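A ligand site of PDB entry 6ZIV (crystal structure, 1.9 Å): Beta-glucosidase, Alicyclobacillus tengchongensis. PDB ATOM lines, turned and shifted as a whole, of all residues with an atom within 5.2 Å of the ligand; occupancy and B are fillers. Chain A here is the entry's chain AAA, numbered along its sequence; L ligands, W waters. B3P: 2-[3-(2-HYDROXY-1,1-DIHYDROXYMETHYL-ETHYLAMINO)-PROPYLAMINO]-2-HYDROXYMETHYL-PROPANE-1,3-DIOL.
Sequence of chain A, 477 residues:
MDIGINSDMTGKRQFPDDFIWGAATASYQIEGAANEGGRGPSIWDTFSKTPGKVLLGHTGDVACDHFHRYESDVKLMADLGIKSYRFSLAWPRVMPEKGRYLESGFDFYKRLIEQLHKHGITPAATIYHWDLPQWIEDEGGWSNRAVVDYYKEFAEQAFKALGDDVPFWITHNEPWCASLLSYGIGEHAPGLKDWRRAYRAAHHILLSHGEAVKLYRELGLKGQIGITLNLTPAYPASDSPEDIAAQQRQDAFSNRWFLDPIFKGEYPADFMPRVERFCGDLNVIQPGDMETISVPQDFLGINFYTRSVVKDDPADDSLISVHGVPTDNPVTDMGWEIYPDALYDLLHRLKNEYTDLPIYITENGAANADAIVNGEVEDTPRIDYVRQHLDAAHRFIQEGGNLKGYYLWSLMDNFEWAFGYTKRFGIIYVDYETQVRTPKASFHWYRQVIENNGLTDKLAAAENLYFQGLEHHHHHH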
ATOM      1  N   GLN A  29      10.658  26.414  12.178  1.00  0.00           N
ATOM      2  CA  GLN A  29      10.380  25.068  12.633  1.00  0.00           C
ATOM      3  C   GLN A  29       9.206  25.037  13.632  1.00  0.00           C
ATOM      4  O   GLN A  29       8.559  23.992  13.755  1.00  0.00           O
ATOM      5  CB  GLN A  29      11.655  24.422  13.176  1.00  0.00           C
ATOM      6  CG  GLN A  29      12.738  24.191  12.134  1.00  0.00           C
ATOM      7  CD  GLN A  29      13.920  23.485  12.725  1.00  0.00           C
ATOM      8  OE1 GLN A  29      14.824  24.122  13.281  1.00  0.00           O
ATOM      9  NE2 GLN A  29      13.931  22.161  12.614  1.00  0.00           N
ATOM     10  N   HIS A 129      18.722  31.308  10.786  1.00  0.00           N
ATOM     11  CA  HIS A 129      18.570  29.866  10.896  1.00  0.00           C
ATOM     12  C   HIS A 129      17.712  29.405   9.704  1.00  0.00           C
ATOM     13  O   HIS A 129      16.710  28.710   9.872  1.00  0.00           O
ATOM     14  CB  HIS A 129      17.971  29.462  12.253  1.00  0.00           C
ATOM     15  CG  HIS A 129      18.180  28.047  12.696  1.00  0.00           C
ATOM     16  ND1 HIS A 129      18.652  27.709  13.953  1.00  0.00           N
ATOM     17  CD2 HIS A 129      17.973  26.882  12.055  1.00  0.00           C
ATOM     18  CE1 HIS A 129      18.714  26.403  14.082  1.00  0.00           C
ATOM     19  NE2 HIS A 129      18.301  25.853  12.902  1.00  0.00           N
ATOM     20  N   TRP A 130      18.114  29.886   8.506  1.00  0.00           N
ATOM     21  CA  TRP A 130      17.867  29.245   7.221  1.00  0.00           C
ATOM     22  C   TRP A 130      16.672  29.856   6.482  1.00  0.00           C
ATOM     23  O   TRP A 130      16.456  29.510   5.317  1.00  0.00           O
ATOM     24  CB  TRP A 130      17.749  27.729   7.323  1.00  0.00           C
ATOM     25  CG  TRP A 130      18.885  27.006   7.981  1.00  0.00           C
ATOM     26  CD1 TRP A 130      20.078  27.516   8.383  1.00  0.00           C
ATOM     27  CD2 TRP A 130      18.941  25.595   8.270  1.00  0.00           C
ATOM     28  NE1 TRP A 130      20.859  26.534   8.917  1.00  0.00           N
ATOM     29  CE2 TRP A 130      20.195  25.339   8.859  1.00  0.00           C
ATOM     30  CE3 TRP A 130      18.050  24.535   8.109  1.00  0.00           C
ATOM     31  CZ2 TRP A 130      20.585  24.060   9.281  1.00  0.00           C
ATOM     32  CZ3 TRP A 130      18.423  23.270   8.515  1.00  0.00           C
ATOM     33  CH2 TRP A 130      19.672  23.043   9.088  1.00  0.00           C
ATOM     34  N   GLU A 174      24.856  26.919  11.499  1.00  0.00           N
ATOM     35  CA  GLU A 174      25.258  25.814  10.641  1.00  0.00           C
ATOM     36  C   GLU A 174      25.484  26.256   9.190  1.00  0.00           C
ATOM     37  O   GLU A 174      24.740  25.862   8.279  1.00  0.00           O
ATOM     38  CB  GLU A 174      24.255  24.673  10.755  1.00  0.00           C
ATOM     39  CG  GLU A 174      24.157  24.136  12.182  1.00  0.00           C
ATOM     40  CD  GLU A 174      23.391  22.822  12.259  1.00  0.00           C
ATOM     41  OE1 GLU A 174      22.830  22.401  11.214  1.00  0.00           O
ATOM     42  OE2 GLU A 174      23.312  22.237  13.349  1.00  0.00           O
ATOM     43  N   TRP A 176      27.506  25.048   7.097  1.00  0.00           N
ATOM     44  CA  TRP A 176      27.618  23.864   6.252  1.00  0.00           C
ATOM     45  C   TRP A 176      26.262  23.476   5.648  1.00  0.00           C
ATOM     46  O   TRP A 176      26.168  23.147   4.460  1.00  0.00           O
ATOM     47  CB  TRP A 176      28.293  22.694   6.980  1.00  0.00           C
ATOM     48  CG  TRP A 176      28.445  21.477   6.112  1.00  0.00           C
ATOM     49  CD1 TRP A 176      29.530  21.152   5.338  1.00  0.00           C
ATOM     50  CD2 TRP A 176      27.473  20.444   5.891  1.00  0.00           C
ATOM     51  NE1 TRP A 176      29.298  19.979   4.680  1.00  0.00           N
ATOM     52  CE2 TRP A 176      28.039  19.521   4.988  1.00  0.00           C
ATOM     53  CE3 TRP A 176      26.200  20.192   6.403  1.00  0.00           C
ATOM     54  CZ2 TRP A 176      27.357  18.379   4.555  1.00  0.00           C
ATOM     55  CZ3 TRP A 176      25.530  19.054   5.985  1.00  0.00           C
ATOM     56  CH2 TRP A 176      26.095  18.171   5.073  1.00  0.00           C
ATOM     57  N   CYS A 177      25.200  23.511   6.465  1.00  0.00           N
ATOM     58  CA  CYS A 177      23.873  23.129   5.992  1.00  0.00           C
ATOM     59  C   CYS A 177      23.299  24.164   5.038  1.00  0.00           C
ATOM     60  O   CYS A 177      22.727  23.812   3.996  1.00  0.00           O
ATOM     61  CB  CYS A 177      22.923  22.947   7.165  1.00  0.00           C
ATOM     62  SG  CYS A 177      23.236  21.414   8.087  1.00  0.00           S
ATOM     63  N   LEU A 181      24.676  21.706   2.008  1.00  0.00           N
ATOM     64  CA  LEU A 181      23.544  20.801   1.956  1.00  0.00           C
ATOM     65  C   LEU A 181      22.404  21.386   1.104  1.00  0.00           C
ATOM     66  O   LEU A 181      21.640  20.647   0.504  1.00  0.00           O
ATOM     67  CB  LEU A 181      23.086  20.498   3.397  1.00  0.00           C
ATOM     68  CG  LEU A 181      21.970  19.453   3.523  1.00  0.00           C
ATOM     69  CD1 LEU A 181      22.453  18.068   3.112  1.00  0.00           C
ATOM     70  CD2 LEU A 181      21.467  19.427   4.955  1.00  0.00           C
ATOM     71  N   GLU A 187      19.348  18.782  -0.457  1.00  0.00           N
ATOM     72  CA  GLU A 187      18.359  18.223   0.455  1.00  0.00           C
ATOM     73  C   GLU A 187      17.512  19.319   1.106  1.00  0.00           C
ATOM     74  O   GLU A 187      16.375  19.080   1.483  1.00  0.00           O
ATOM     75  CB  GLU A 187      19.001  17.401   1.573  1.00  0.00           C
ATOM     76  CG  GLU A 187      19.340  15.980   1.154  1.00  0.00           C
ATOM     77  CD  GLU A 187      20.099  15.214   2.219  1.00  0.00           C
ATOM     78  OE1 GLU A 187      19.853  15.452   3.435  1.00  0.00           O
ATOM     79  OE2 GLU A 187      20.960  14.386   1.837  1.00  0.00           O
ATOM     80  N   HIS A 188      18.115  20.507   1.279  1.00  0.00           N
ATOM     81  CA  HIS A 188      17.491  21.639   1.953  1.00  0.00           C
ATOM     82  C   HIS A 188      17.326  22.824   1.005  1.00  0.00           C
ATOM     83  O   HIS A 188      18.047  22.963   0.021  1.00  0.00           O
ATOM     84  CB  HIS A 188      18.359  22.062   3.148  1.00  0.00           C
ATOM     85  CG  HIS A 188      18.256  21.191   4.367  1.00  0.00           C
ATOM     86  ND1 HIS A 188      18.866  21.531   5.563  1.00  0.00           N
ATOM     87  CD2 HIS A 188      17.611  20.018   4.573  1.00  0.00           C
ATOM     88  CE1 HIS A 188      18.622  20.604   6.455  1.00  0.00           C
ATOM     89  NE2 HIS A 188      17.852  19.669   5.883  1.00  0.00           N
ATOM     90  N   ASN A 230      27.784  23.343  12.987  1.00  0.00           N
ATOM     91  CA  ASN A 230      27.616  21.912  13.159  1.00  0.00           C
ATOM     92  C   ASN A 230      28.946  21.242  12.825  1.00  0.00           C
ATOM     93  O   ASN A 230      29.541  21.501  11.779  1.00  0.00           O
ATOM     94  CB  ASN A 230      26.452  21.310  12.357  1.00  0.00           C
ATOM     95  CG  ASN A 230      26.505  21.636  10.876  1.00  0.00           C
ATOM     96  OD1 ASN A 230      26.843  22.764  10.494  1.00  0.00           O
ATOM     97  ND2 ASN A 230      26.162  20.653  10.049  1.00  0.00           N
ATOM     98  N   TYR A 305      25.967  16.047  17.122  1.00  0.00           N
ATOM     99  CA  TYR A 305      24.963  14.999  17.097  1.00  0.00           C
ATOM    100  C   TYR A 305      25.625  13.634  16.956  1.00  0.00           C
ATOM    101  O   TYR A 305      25.220  12.696  17.651  1.00  0.00           O
ATOM    102  CB  TYR A 305      23.917  15.242  16.027  1.00  0.00           C
ATOM    103  CG  TYR A 305      22.996  16.401  16.332  1.00  0.00           C
ATOM    104  CD1 TYR A 305      23.320  17.681  15.949  1.00  0.00           C
ATOM    105  CD2 TYR A 305      21.827  16.208  17.045  1.00  0.00           C
ATOM    106  CE1 TYR A 305      22.468  18.751  16.222  1.00  0.00           C
ATOM    107  CE2 TYR A 305      20.959  17.254  17.325  1.00  0.00           C
ATOM    108  CZ  TYR A 305      21.287  18.532  16.900  1.00  0.00           C
ATOM    109  OH  TYR A 305      20.443  19.573  17.175  1.00  0.00           O
ATOM    110  N   MET A 334      16.993   8.729  13.753  1.00  0.00           N
ATOM    111  CA  MET A 334      17.450   9.259  12.474  1.00  0.00           C
ATOM    112  C   MET A 334      18.398   8.259  11.811  1.00  0.00           C
ATOM    113  O   MET A 334      18.782   8.440  10.665  1.00  0.00           O
ATOM    114  CB  MET A 334      18.202  10.586  12.638  1.00  0.00           C
ATOM    115  CG  MET A 334      17.362  11.720  13.209  1.00  0.00           C
ATOM    116  SD  MET A 334      15.802  12.095  12.260  1.00  0.00           S
ATOM    117  CE  MET A 334      16.488  12.799  10.758  1.00  0.00           C
ATOM    118  N   TRP A 336      21.435   7.849  13.081  1.00  0.00           N
ATOM    119  CA  TRP A 336      22.765   8.355  13.378  1.00  0.00           C
ATOM    120  C   TRP A 336      23.379   7.601  14.539  1.00  0.00           C
ATOM    121  O   TRP A 336      22.696   7.359  15.545  1.00  0.00           O
ATOM    122  CB  TRP A 336      22.758   9.857  13.660  1.00  0.00           C
ATOM    123  CG  TRP A 336      21.994  10.699  12.671  1.00  0.00           C
ATOM    124  CD1 TRP A 336      21.714  10.400  11.375  1.00  0.00           C
ATOM    125  CD2 TRP A 336      21.458  12.018  12.907  1.00  0.00           C
ATOM    126  NE1 TRP A 336      21.009  11.419  10.798  1.00  0.00           N
ATOM    127  CE2 TRP A 336      20.838  12.428  11.708  1.00  0.00           C
ATOM    128  CE3 TRP A 336      21.390  12.850  14.027  1.00  0.00           C
ATOM    129  CZ2 TRP A 336      20.200  13.658  11.594  1.00  0.00           C
ATOM    130  CZ3 TRP A 336      20.797  14.080  13.904  1.00  0.00           C
ATOM    131  CH2 TRP A 336      20.203  14.475  12.702  1.00  0.00           C
ATOM    132  N   GLU A 363      23.519  23.186  20.337  1.00  0.00           N
ATOM    133  CA  GLU A 363      22.526  22.148  20.107  1.00  0.00           C
ATOM    134  C   GLU A 363      23.157  20.792  20.375  1.00  0.00           C
ATOM    135  O   GLU A 363      24.307  20.561  20.018  1.00  0.00           O
ATOM    136  CB  GLU A 363      22.074  22.085  18.640  1.00  0.00           C
ATOM    137  CG  GLU A 363      21.291  23.287  18.168  1.00  0.00           C
ATOM    138  CD  GLU A 363      20.756  23.156  16.744  1.00  0.00           C
ATOM    139  OE1 GLU A 363      20.621  22.009  16.275  1.00  0.00           O
ATOM    140  OE2 GLU A 363      20.485  24.183  16.124  1.00  0.00           O
ATOM    141  N   TRP A 409      18.594  20.433  21.922  1.00  0.00           N
ATOM    142  CA  TRP A 409      17.668  20.454  20.789  1.00  0.00           C
ATOM    143  C   TRP A 409      16.692  19.279  20.929  1.00  0.00           C
ATOM    144  O   TRP A 409      17.136  18.135  20.875  1.00  0.00           O
ATOM    145  CB  TRP A 409      18.415  20.370  19.454  1.00  0.00           C
ATOM    146  CG  TRP A 409      17.456  20.505  18.305  1.00  0.00           C
ATOM    147  CD1 TRP A 409      16.722  19.525  17.703  1.00  0.00           C
ATOM    148  CD2 TRP A 409      17.035  21.745  17.710  1.00  0.00           C
ATOM    149  NE1 TRP A 409      15.880  20.073  16.759  1.00  0.00           N
ATOM    150  CE2 TRP A 409      16.049  21.433  16.747  1.00  0.00           C
ATOM    151  CE3 TRP A 409      17.410  23.074  17.894  1.00  0.00           C
ATOM    152  CZ2 TRP A 409      15.468  22.404  15.944  1.00  0.00           C
ATOM    153  CZ3 TRP A 409      16.812  24.043  17.118  1.00  0.00           C
ATOM    154  CH2 TRP A 409      15.855  23.707  16.151  1.00  0.00           C
ATOM    155  N   ASN A 414       8.929  19.565  16.363  1.00  0.00           N
ATOM    156  CA  ASN A 414       8.846  20.657  15.414  1.00  0.00           C
ATOM    157  C   ASN A 414       9.040  20.133  13.975  1.00  0.00           C
ATOM    158  O   ASN A 414       9.238  18.929  13.753  1.00  0.00           O
ATOM    159  CB  ASN A 414       9.817  21.782  15.781  1.00  0.00           C
ATOM    160  CG  ASN A 414      11.270  21.377  15.736  1.00  0.00           C
ATOM    161  OD1 ASN A 414      11.772  21.015  14.675  1.00  0.00           O
ATOM    162  ND2 ASN A 414      11.951  21.452  16.880  1.00  0.00           N
ATOM    163  N   GLU A 416      10.854  19.091  11.097  1.00  0.00           N
ATOM    164  CA  GLU A 416      12.201  18.549  10.924  1.00  0.00           C
ATOM    165  C   GLU A 416      12.621  18.634   9.452  1.00  0.00           C
ATOM    166  O   GLU A 416      12.960  17.623   8.825  1.00  0.00           O
ATOM    167  CB  GLU A 416      12.249  17.122  11.470  1.00  0.00           C
ATOM    168  CG  GLU A 416      13.595  16.440  11.359  1.00  0.00           C
ATOM    169  CD  GLU A 416      14.771  17.206  11.942  1.00  0.00           C
ATOM    170  OE1 GLU A 416      14.577  17.965  12.895  1.00  0.00           O
ATOM    171  OE2 GLU A 416      15.883  17.057  11.399  1.00  0.00           O
ATOM    172  N   TRP A 417      12.590  19.869   8.916  1.00  0.00           N
ATOM    173  CA  TRP A 417      13.073  20.196   7.591  1.00  0.00           C
ATOM    174  C   TRP A 417      12.557  19.208   6.552  1.00  0.00           C
ATOM    175  O   TRP A 417      11.341  19.109   6.373  1.00  0.00           O
ATOM    176  CB  TRP A 417      14.597  20.369   7.603  1.00  0.00           C
ATOM    177  CG  TRP A 417      15.044  21.388   8.598  1.00  0.00           C
ATOM    178  CD1 TRP A 417      15.832  21.199   9.700  1.00  0.00           C
ATOM    179  CD2 TRP A 417      14.703  22.791   8.597  1.00  0.00           C
ATOM    180  NE1 TRP A 417      16.015  22.390  10.366  1.00  0.00           N
ATOM    181  CE2 TRP A 417      15.333  23.378   9.715  1.00  0.00           C
ATOM    182  CE3 TRP A 417      13.927  23.598   7.742  1.00  0.00           C
ATOM    183  CZ2 TRP A 417      15.224  24.731   9.999  1.00  0.00           C
ATOM    184  CZ3 TRP A 417      13.819  24.941   8.027  1.00  0.00           C
ATOM    185  CH2 TRP A 417      14.443  25.487   9.160  1.00  0.00           C
ATOM    186  N   PHE A 425      12.229  15.540  17.961  1.00  0.00           N
ATOM    187  CA  PHE A 425      13.449  15.823  18.710  1.00  0.00           C
ATOM    188  C   PHE A 425      13.130  16.515  20.036  1.00  0.00           C
ATOM    189  O   PHE A 425      14.055  16.830  20.799  1.00  0.00           O
ATOM    190  CB  PHE A 425      14.367  16.765  17.925  1.00  0.00           C
ATOM    191  CG  PHE A 425      15.305  16.091  16.940  1.00  0.00           C
ATOM    192  CD1 PHE A 425      14.891  15.801  15.643  1.00  0.00           C
ATOM    193  CD2 PHE A 425      16.623  15.793  17.296  1.00  0.00           C
ATOM    194  CE1 PHE A 425      15.758  15.198  14.748  1.00  0.00           C
ATOM    195  CE2 PHE A 425      17.492  15.220  16.378  1.00  0.00           C
ATOM    196  CZ  PHE A 425      17.055  14.927  15.100  1.00  0.00           C
HETATM  197  C1  B3P L   1      22.275  18.389  12.731  1.00  0.00           C
HETATM  198  C2  B3P L   1      22.260  18.553  11.227  1.00  0.00           C
HETATM  199  C3  B3P L   1      21.014  18.924  13.420  1.00  0.00           C
HETATM  200  N1  B3P L   1      19.850  19.090  12.539  1.00  0.00           N
HETATM  201  C4  B3P L   1      18.540  19.202  13.245  1.00  0.00           C
HETATM  202  C5  B3P L   1      18.035  17.844  13.725  1.00  0.00           C
HETATM  203  C6  B3P L   1      17.489  19.814  12.317  1.00  0.00           C
HETATM  204  C7  B3P L   1      18.626  20.011  14.549  1.00  0.00           C
HETATM  205  N2  B3P L   1      21.839  17.297  10.608  1.00  0.00           N
HETATM  206  C8  B3P L   1      21.376  17.348   9.185  1.00  0.00           C
HETATM  207  C9  B3P L   1      22.604  17.388   8.285  1.00  0.00           C
HETATM  208  C10 B3P L   1      20.525  18.584   8.861  1.00  0.00           C
HETATM  209  C11 B3P L   1      20.570  16.101   8.863  1.00  0.00           C
HETATM  210  O1  B3P L   1      23.774  16.954   8.971  1.00  0.00           O
HETATM  211  O2  B3P L   1      19.335  18.710   9.638  1.00  0.00           O
HETATM  212  O3  B3P L   1      20.784  15.762   7.490  1.00  0.00           O
HETATM  213  O4  B3P L   1      18.204  16.841  12.750  1.00  0.00           O
HETATM  214  O5  B3P L   1      16.269  19.878  13.043  1.00  0.00           O
HETATM  215  O6  B3P L   1      18.818  21.415  14.352  1.00  0.00           O
HETATM  216  O   HOH W   1      20.751  23.497  13.689  1.00  0.00           O
HETATM  217  O   HOH W   2      17.265  16.808   9.018  1.00  0.00           O
HETATM  218  O   HOH W   3      17.691  23.036  12.749  1.00  0.00           O
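OE1 of Glu 416 is in hydrogen-bond range of O5 of the ligand (2.6 Å). The side-chain carboxylate (OE1) of Glu 363 lies within hydrogen-bond range of an oxygen (O6) of the ligand (2.7 Å). The side-chain amide nitrogen (NE2) of Gln 29 sits at hydrogen-bond distance from an oxygen (O5) of the ligand (3.3 Å).
OH of Tyr 305 is in hydrogen-bond range of OE1 of Glu 363 (2.6 Å). The side-chain amide nitrogen of Gln 29 lies close to the indole nitrogen of Trp 417, 3.1 Å away. The side-chain amide nitrogen of Gln 29 lies within hydrogen-bond range of the side-chain amide oxygen of Asn 414, at 3.2 Å. SG of Cys 177 sits at hydrogen-bond distance from OE1 of Glu 174, 3.3 Å away. SG of Cys 177 sits at hydrogen-bond distance from ND2 of Asn 230.
Glu 174 touches the ligand. Cys 177 touches the ligand. His 188 touches the ligand (CE1 to C10, 3.7 Å). CE1 of Tyr 305 touches C3 of the ligand, 3.2 Å away. Trp 336 touches the ligand. Trp 409 touches the ligand. Trp 417 touches the ligand (CD1 to C6, 3.4 Å). Phe 425 touches the ligand (CZ to O4, 3.2 Å). Hydrophobic or aromatic side chains within 4 Å of the ligand: His 188, Tyr 305, Trp 336, Trp 409, Trp 417 and Phe 425. 11 residues have an atom within 4 Å of the ligand: Gln 29, Glu 174, Cys 177, His 188, Tyr 305, Trp 336, Glu 363, Trp 409, Glu 416, Trp 417 and Phe 425.
Water W3 lies within hydrogen-bond range of an oxygen (O6) of the ligand (2.5 Å), a ring nitrogen (NE2) of His 129 (2.9 Å), the indole nitrogen (NE1) of Trp 417 (3.0 Å) and the side-chain amide oxygen (OE1) of Gln 29 (3.1 Å). Water W2 lies within hydrogen-bond range of the side-chain carboxylate of Glu 416 (2.8 Å) and an oxygen (O2) of the ligand (2.9 Å). Water W1 lies within hydrogen-bond range of OE2 of Glu 363 (2.5 Å), OE2 of Glu 174 (2.9 Å), O6 of the ligand (2.9 Å) and NE2 of His 129 (3.5 Å).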
